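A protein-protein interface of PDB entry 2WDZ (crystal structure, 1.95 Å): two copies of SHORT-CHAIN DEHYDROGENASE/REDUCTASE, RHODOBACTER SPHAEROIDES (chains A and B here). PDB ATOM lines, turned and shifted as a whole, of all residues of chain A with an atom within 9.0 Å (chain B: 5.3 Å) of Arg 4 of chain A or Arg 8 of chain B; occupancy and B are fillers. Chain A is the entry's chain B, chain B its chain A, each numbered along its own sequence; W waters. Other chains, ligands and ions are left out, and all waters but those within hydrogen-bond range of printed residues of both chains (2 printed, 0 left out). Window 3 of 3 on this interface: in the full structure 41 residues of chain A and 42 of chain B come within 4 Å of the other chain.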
ATOM      1  N   MET A   1     -11.250  22.132 -10.373  1.00  0.00           N
ATOM      2  CA  MET A   1      -9.826  22.518 -10.634  1.00  0.00           C
ATOM      3  C   MET A   1      -9.702  23.983 -10.996  1.00  0.00           C
ATOM      4  O   MET A   1     -10.427  24.467 -11.864  1.00  0.00           O
ATOM      5  CB  MET A   1      -9.219  21.680 -11.766  1.00  0.00           C
ATOM      6  CG  MET A   1      -7.703  21.632 -11.690  1.00  0.00           C
ATOM      7  SD  MET A   1      -6.881  20.435 -12.754  1.00  0.00           S
ATOM      8  CE  MET A   1      -7.052  18.846 -11.944  1.00  0.00           C
ATOM      9  N   ASP A   2      -8.781  24.669 -10.323  1.00  0.00           N
ATOM     10  CA  ASP A   2      -8.369  26.016 -10.685  1.00  0.00           C
ATOM     11  C   ASP A   2      -6.961  25.979 -11.325  1.00  0.00           C
ATOM     12  O   ASP A   2      -5.954  25.876 -10.624  1.00  0.00           O
ATOM     13  CB  ASP A   2      -8.403  26.905  -9.434  1.00  0.00           C
ATOM     14  CG  ASP A   2      -7.867  28.309  -9.689  1.00  0.00           C
ATOM     15  OD1 ASP A   2      -7.895  28.771 -10.853  1.00  0.00           O
ATOM     16  OD2 ASP A   2      -7.410  28.960  -8.721  1.00  0.00           O
ATOM     17  N   TYR A   3      -6.901  26.068 -12.662  1.00  0.00           N
ATOM     18  CA  TYR A   3      -5.654  25.822 -13.416  1.00  0.00           C
ATOM     19  C   TYR A   3      -4.509  26.745 -13.044  1.00  0.00           C
ATOM     20  O   TYR A   3      -3.311  26.432 -13.255  1.00  0.00           O
ATOM     21  CB  TYR A   3      -5.910  25.874 -14.915  1.00  0.00           C
ATOM     22  CG  TYR A   3      -6.784  24.728 -15.344  1.00  0.00           C
ATOM     23  CD1 TYR A   3      -6.257  23.422 -15.475  1.00  0.00           C
ATOM     24  CD2 TYR A   3      -8.151  24.924 -15.593  1.00  0.00           C
ATOM     25  CE1 TYR A   3      -7.094  22.342 -15.885  1.00  0.00           C
ATOM     26  CE2 TYR A   3      -8.977  23.873 -15.978  1.00  0.00           C
ATOM     27  CZ  TYR A   3      -8.449  22.586 -16.132  1.00  0.00           C
ATOM     28  OH  TYR A   3      -9.284  21.564 -16.527  1.00  0.00           O
ATOM     29  N   ARG A   4      -4.887  27.866 -12.448  1.00  0.00           N
ATOM     30  CA  ARG A   4      -3.950  28.947 -12.185  1.00  0.00           C
ATOM     31  C   ARG A   4      -2.960  28.603 -11.090  1.00  0.00           C
ATOM     32  O   ARG A   4      -1.775  28.992 -11.139  1.00  0.00           O
ATOM     33  CB  ARG A   4      -4.723  30.212 -11.868  1.00  0.00           C
ATOM     34  CG  ARG A   4      -4.916  31.049 -13.105  1.00  0.00           C
ATOM     35  CD  ARG A   4      -3.562  31.663 -13.442  1.00  0.00           C
ATOM     36  NE  ARG A   4      -3.702  32.978 -14.070  1.00  0.00           N
ATOM     37  CZ  ARG A   4      -3.818  34.122 -13.406  1.00  0.00           C
ATOM     38  NH1 ARG A   4      -3.821  34.124 -12.079  1.00  0.00           N
ATOM     39  NH2 ARG A   4      -3.939  35.263 -14.076  1.00  0.00           N
ATOM     40  N   THR A   5      -3.446  27.835 -10.131  1.00  0.00           N
ATOM     41  CA  THR A   5      -2.669  27.495  -8.981  1.00  0.00           C
ATOM     42  C   THR A   5      -2.575  25.963  -8.800  1.00  0.00           C
ATOM     43  O   THR A   5      -2.038  25.512  -7.818  1.00  0.00           O
ATOM     44  CB  THR A   5      -3.271  28.182  -7.734  1.00  0.00           C
ATOM     45  OG1 THR A   5      -4.599  27.689  -7.503  1.00  0.00           O
ATOM     46  CG2 THR A   5      -3.292  29.730  -7.925  1.00  0.00           C
ATOM     47  N   VAL A   6      -3.058  25.184  -9.777  1.00  0.00           N
ATOM     48  CA  VAL A   6      -3.095  23.708  -9.653  1.00  0.00           C
ATOM     49  C   VAL A   6      -1.698  23.050  -9.691  1.00  0.00           C
ATOM     50  O   VAL A   6      -1.559  21.883  -9.321  1.00  0.00           O
ATOM     51  CB  VAL A   6      -4.061  23.038 -10.693  1.00  0.00           C
ATOM     52  CG1 VAL A   6      -3.380  22.863 -12.040  1.00  0.00           C
ATOM     53  CG2 VAL A   6      -4.546  21.692 -10.161  1.00  0.00           C
ATOM     54  N   PHE A   7      -0.687  23.807 -10.135  1.00  0.00           N
ATOM     55  CA  PHE A   7       0.688  23.315 -10.205  1.00  0.00           C
ATOM     56  C   PHE A   7       1.592  23.634  -8.954  1.00  0.00           C
ATOM     57  O   PHE A   7       2.792  23.263  -8.903  1.00  0.00           O
ATOM     58  CB  PHE A   7       1.340  23.844 -11.440  1.00  0.00           C
ATOM     59  CG  PHE A   7       0.724  23.356 -12.713  1.00  0.00           C
ATOM     60  CD1 PHE A   7       1.088  22.108 -13.237  1.00  0.00           C
ATOM     61  CD2 PHE A   7      -0.152  24.179 -13.428  1.00  0.00           C
ATOM     62  CE1 PHE A   7       0.567  21.676 -14.439  1.00  0.00           C
ATOM     63  CE2 PHE A   7      -0.679  23.755 -14.638  1.00  0.00           C
ATOM     64  CZ  PHE A   7      -0.310  22.492 -15.150  1.00  0.00           C
ATOM     65  N   ARG A   8       0.973  24.307  -7.988  1.00  0.00           N
ATOM     66  CA  ARG A   8       1.579  24.739  -6.764  1.00  0.00           C
ATOM     67  C   ARG A   8       1.517  23.644  -5.688  1.00  0.00           C
ATOM     68  O   ARG A   8       0.743  22.672  -5.785  1.00  0.00           O
ATOM     69  CB  ARG A   8       0.855  26.007  -6.282  1.00  0.00           C
ATOM     70  CG  ARG A   8       0.803  27.179  -7.313  1.00  0.00           C
ATOM     71  CD  ARG A   8       1.909  28.145  -7.101  1.00  0.00           C
ATOM     72  NE  ARG A   8       2.062  28.466  -5.678  1.00  0.00           N
ATOM     73  CZ  ARG A   8       3.063  29.166  -5.144  1.00  0.00           C
ATOM     74  NH1 ARG A   8       4.044  29.653  -5.898  1.00  0.00           N
ATOM     75  NH2 ARG A   8       3.086  29.362  -3.836  1.00  0.00           N
ATOM     76  N   ASP A  10       1.450  24.579  -2.289  1.00  0.00           N
ATOM     77  CA  ASP A  10       1.223  25.379  -1.082  1.00  0.00           C
ATOM     78  C   ASP A  10       0.725  24.519   0.061  1.00  0.00           C
ATOM     79  O   ASP A  10      -0.190  23.709  -0.100  1.00  0.00           O
ATOM     80  CB  ASP A  10       0.260  26.526  -1.375  1.00  0.00           C
ATOM     81  CG  ASP A  10       0.911  27.625  -2.186  1.00  0.00           C
ATOM     82  OD1 ASP A  10       1.800  28.328  -1.662  1.00  0.00           O
ATOM     83  OD2 ASP A  10       0.521  27.769  -3.357  1.00  0.00           O
ATOM     84  N   ARG B   4       6.930  29.691 -11.079  1.00  0.00           N
ATOM     85  CA  ARG B   4       5.571  30.071 -10.738  1.00  0.00           C
ATOM     86  C   ARG B   4       4.756  30.350 -11.975  1.00  0.00           C
ATOM     87  O   ARG B   4       3.526  30.384 -11.912  1.00  0.00           O
ATOM     88  CB  ARG B   4       5.550  31.304  -9.865  1.00  0.00           C
ATOM     89  CG  ARG B   4       5.428  31.033  -8.397  1.00  0.00           C
ATOM     90  CD  ARG B   4       4.818  32.295  -7.765  1.00  0.00           C
ATOM     91  NE  ARG B   4       5.694  32.779  -6.709  1.00  0.00           N
ATOM     92  CZ  ARG B   4       6.954  33.186  -6.899  1.00  0.00           C
ATOM     93  NH1 ARG B   4       7.516  33.168  -8.115  1.00  0.00           N
ATOM     94  NH2 ARG B   4       7.665  33.605  -5.863  1.00  0.00           N
ATOM     95  N   THR B   5       5.428  30.592 -13.090  1.00  0.00           N
ATOM     96  CA  THR B   5       4.704  30.842 -14.325  1.00  0.00           C
ATOM     97  C   THR B   5       5.186  29.961 -15.507  1.00  0.00           C
ATOM     98  O   THR B   5       4.756  30.144 -16.617  1.00  0.00           O
ATOM     99  CB  THR B   5       4.769  32.331 -14.698  1.00  0.00           C
ATOM    100  OG1 THR B   5       6.141  32.690 -14.946  1.00  0.00           O
ATOM    101  CG2 THR B   5       4.105  33.254 -13.529  1.00  0.00           C
ATOM    102  N   VAL B   6       6.032  28.968 -15.225  1.00  0.00           N
ATOM    103  CA  VAL B   6       6.572  28.082 -16.265  1.00  0.00           C
ATOM    104  C   VAL B   6       5.467  27.329 -16.999  1.00  0.00           C
ATOM    105  O   VAL B   6       5.634  27.001 -18.171  1.00  0.00           O
ATOM    106  CB  VAL B   6       7.668  27.118 -15.736  1.00  0.00           C
ATOM    107  CG1 VAL B   6       7.057  25.982 -14.832  1.00  0.00           C
ATOM    108  CG2 VAL B   6       8.557  26.614 -16.940  1.00  0.00           C
ATOM    109  N   PHE B   7       4.354  27.043 -16.303  1.00  0.00           N
ATOM    110  CA  PHE B   7       3.248  26.307 -16.881  1.00  0.00           C
ATOM    111  C   PHE B   7       2.252  27.230 -17.614  1.00  0.00           C
ATOM    112  O   PHE B   7       1.230  26.762 -18.053  1.00  0.00           O
ATOM    113  CB  PHE B   7       2.489  25.487 -15.784  1.00  0.00           C
ATOM    114  CG  PHE B   7       3.374  24.546 -15.016  1.00  0.00           C
ATOM    115  CD1 PHE B   7       3.738  23.306 -15.536  1.00  0.00           C
ATOM    116  CD2 PHE B   7       3.887  24.929 -13.795  1.00  0.00           C
ATOM    117  CE1 PHE B   7       4.597  22.445 -14.825  1.00  0.00           C
ATOM    118  CE2 PHE B   7       4.738  24.057 -13.036  1.00  0.00           C
ATOM    119  CZ  PHE B   7       5.093  22.812 -13.566  1.00  0.00           C
ATOM    120  N   ARG B   8       2.528  28.526 -17.693  1.00  0.00           N
ATOM    121  CA  ARG B   8       1.593  29.480 -18.306  1.00  0.00           C
ATOM    122  C   ARG B   8       1.735  29.467 -19.824  1.00  0.00           C
ATOM    123  O   ARG B   8       2.789  29.058 -20.367  1.00  0.00           O
ATOM    124  CB  ARG B   8       1.828  30.888 -17.783  1.00  0.00           C
ATOM    125  CG  ARG B   8       1.365  31.111 -16.309  1.00  0.00           C
ATOM    126  CD  ARG B   8      -0.156  31.370 -16.139  1.00  0.00           C
ATOM    127  NE  ARG B   8      -0.557  32.646 -16.763  1.00  0.00           N
ATOM    128  CZ  ARG B   8      -1.811  33.078 -16.908  1.00  0.00           C
ATOM    129  NH1 ARG B   8      -2.820  32.353 -16.456  1.00  0.00           N
ATOM    130  NH2 ARG B   8      -2.057  34.241 -17.499  1.00  0.00           N
ATOM    131  N   LEU B   9       0.698  29.940 -20.509  1.00  0.00           N
ATOM    132  CA  LEU B   9       0.760  30.058 -21.946  1.00  0.00           C
ATOM    133  C   LEU B   9       0.618  31.526 -22.429  1.00  0.00           C
ATOM    134  O   LEU B   9      -0.017  31.796 -23.445  1.00  0.00           O
ATOM    135  CB  LEU B   9      -0.293  29.161 -22.595  1.00  0.00           C
ATOM    136  CG  LEU B   9      -0.274  27.658 -22.217  1.00  0.00           C
ATOM    137  CD1 LEU B   9      -1.374  26.941 -22.965  1.00  0.00           C
ATOM    138  CD2 LEU B   9       0.999  26.985 -22.576  1.00  0.00           C
ATOM    139  N   ASP B  10       1.197  32.461 -21.680  1.00  0.00           N
ATOM    140  CA  ASP B  10       0.911  33.865 -21.960  1.00  0.00           C
ATOM    141  C   ASP B  10       1.387  34.277 -23.329  1.00  0.00           C
ATOM    142  O   ASP B  10       2.482  33.906 -23.740  1.00  0.00           O
ATOM    143  CB  ASP B  10       1.481  34.774 -20.887  1.00  0.00           C
ATOM    144  CG  ASP B  10       0.783  34.597 -19.583  1.00  0.00           C
ATOM    145  OD1 ASP B  10      -0.481  34.530 -19.532  1.00  0.00           O
ATOM    146  OD2 ASP B  10       1.522  34.528 -18.586  1.00  0.00           O
ATOM    147  N   ALA B  33      -7.501  29.799 -19.269  1.00  0.00           N
ATOM    148  CA  ALA B  33      -7.104  30.188 -17.915  1.00  0.00           C
ATOM    149  C   ALA B  33      -5.593  30.403 -17.736  1.00  0.00           C
ATOM    150  O   ALA B  33      -5.199  31.104 -16.803  1.00  0.00           O
ATOM    151  CB  ALA B  33      -7.664  29.170 -16.864  1.00  0.00           C
ATOM    152  N   SER B  34      -4.770  29.804 -18.603  1.00  0.00           N
ATOM    153  CA  SER B  34      -3.303  29.965 -18.595  1.00  0.00           C
ATOM    154  C   SER B  34      -2.832  31.078 -19.535  1.00  0.00           C
ATOM    155  O   SER B  34      -1.625  31.234 -19.795  1.00  0.00           O
ATOM    156  CB  SER B  34      -2.569  28.630 -18.876  1.00  0.00           C
ATOM    157  OG  SER B  34      -3.127  27.587 -18.079  1.00  0.00           O
ATOM    158  N   GLY B  35      -3.769  31.888 -19.989  1.00  0.00           N
ATOM    159  CA  GLY B  35      -3.399  33.064 -20.758  1.00  0.00           C
ATOM    160  C   GLY B  35      -3.271  32.933 -22.258  1.00  0.00           C
ATOM    161  O   GLY B  35      -2.871  33.905 -22.906  1.00  0.00           O
ATOM    162  N   SER B 234       3.024  23.440 -22.445  1.00  0.00           N
ATOM    163  CA  SER B 234       3.750  24.610 -21.901  1.00  0.00           C
ATOM    164  C   SER B 234       5.288  24.537 -21.946  1.00  0.00           C
ATOM    165  O   SER B 234       5.856  23.453 -22.091  1.00  0.00           O
ATOM    166  CB  SER B 234       3.357  24.854 -20.456  1.00  0.00           C
ATOM    167  OG  SER B 234       3.868  23.838 -19.663  1.00  0.00           O
ATOM    168  N   PRO B 235       5.953  25.695 -21.712  1.00  0.00           N
ATOM    169  CA  PRO B 235       7.409  25.702 -21.522  1.00  0.00           C
ATOM    170  C   PRO B 235       7.936  24.765 -20.430  1.00  0.00           C
ATOM    171  O   PRO B 235       9.134  24.456 -20.430  1.00  0.00           O
ATOM    172  CB  PRO B 235       7.721  27.174 -21.148  1.00  0.00           C
ATOM    173  CG  PRO B 235       6.565  27.966 -21.778  1.00  0.00           C
ATOM    174  CD  PRO B 235       5.375  27.051 -21.601  1.00  0.00           C
HETATM  175  O   HOH W   1      -2.119  36.741 -15.426  1.00  0.00           O
HETATM  176  O   HOH W   2       2.908  32.819  -5.233  1.00  0.00           O
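Arg 4 of chain A touches Arg 8 of chain B, and with the chains exchanged Arg 8 of chain A touches Arg 4 of chain B. Phe 7 of chain B touches its own counterpart, Phe 7 of chain A.
Of the 12 printed residues of chain B, 4 touch a printed residue of chain A. Printed residues of chain B that touch a printed residue of chain A: Arg 4, Phe 7, Arg 8 and Ala 33. Hydrophobic or aromatic side chains of chain B that line the printed part of chain A: Phe 7.
Arg 4 of chain A touches two residues of chain B. Thr 5 of chain A touches none of the printed residues of chain B. Printed residues of chain B within 4 Å of Phe 7 of chain A: Phe 7 (3.6 Å). Of the printed residues of chain B, Arg 8 of chain A touches Arg 4 (3.2 Å). Of the printed residues of chain A, Arg 4 of chain B touches Arg 8. Of chain A, only Arg 4 comes within 4 Å of Arg 8 of chain B. Printed residues of chain A within 4 Å of Ala 33 of chain B: Arg 4. Ser 234 of chain B touches none of the printed residues of chain A. The nearest printed residue of chain B that does not touch Phe 7 of chain A is Ser 34 of chain B (5.7 Å).
Water W1 lies within hydrogen-bond range of NH2 of Arg 4 of chain A (2.7 Å) and NH2 of Arg 8 of chain B (3.2 Å). Water W2 bridges the guanidinium group (NE) of Arg 4 of chain B (3.2 Å) and the guanidinium group (NH1) of Arg 8 of chain A (3.4 Å).
The guanidinium group (NH1) of Arg 8 of chain B lies close to the guanidinium group (NE) of Arg 4 of chain A, 2.6 Å away.
OD1 of Asp 10 of chain B is in salt-bridge range of NH2 of Arg 8 of chain B (2.6 Å). NH1 of Arg 8 of chain B is in hydrogen-bond range of O of Ala 33 of chain B, 2.7 Å away. OD1 of Asp 10 of chain A lies within salt-bridge range of NH2 of Arg 8 of chain A, 2.7 Å away.
Among the printed residues, merely in contact across the chains: Arg 8 of chain A with Arg 4 of chain B (3.2 Å), Phe 7 of chain A with Phe 7 of chain B (3.6 Å) and Arg 4 of chain A with Ala 33 of chain B (3.6 Å).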
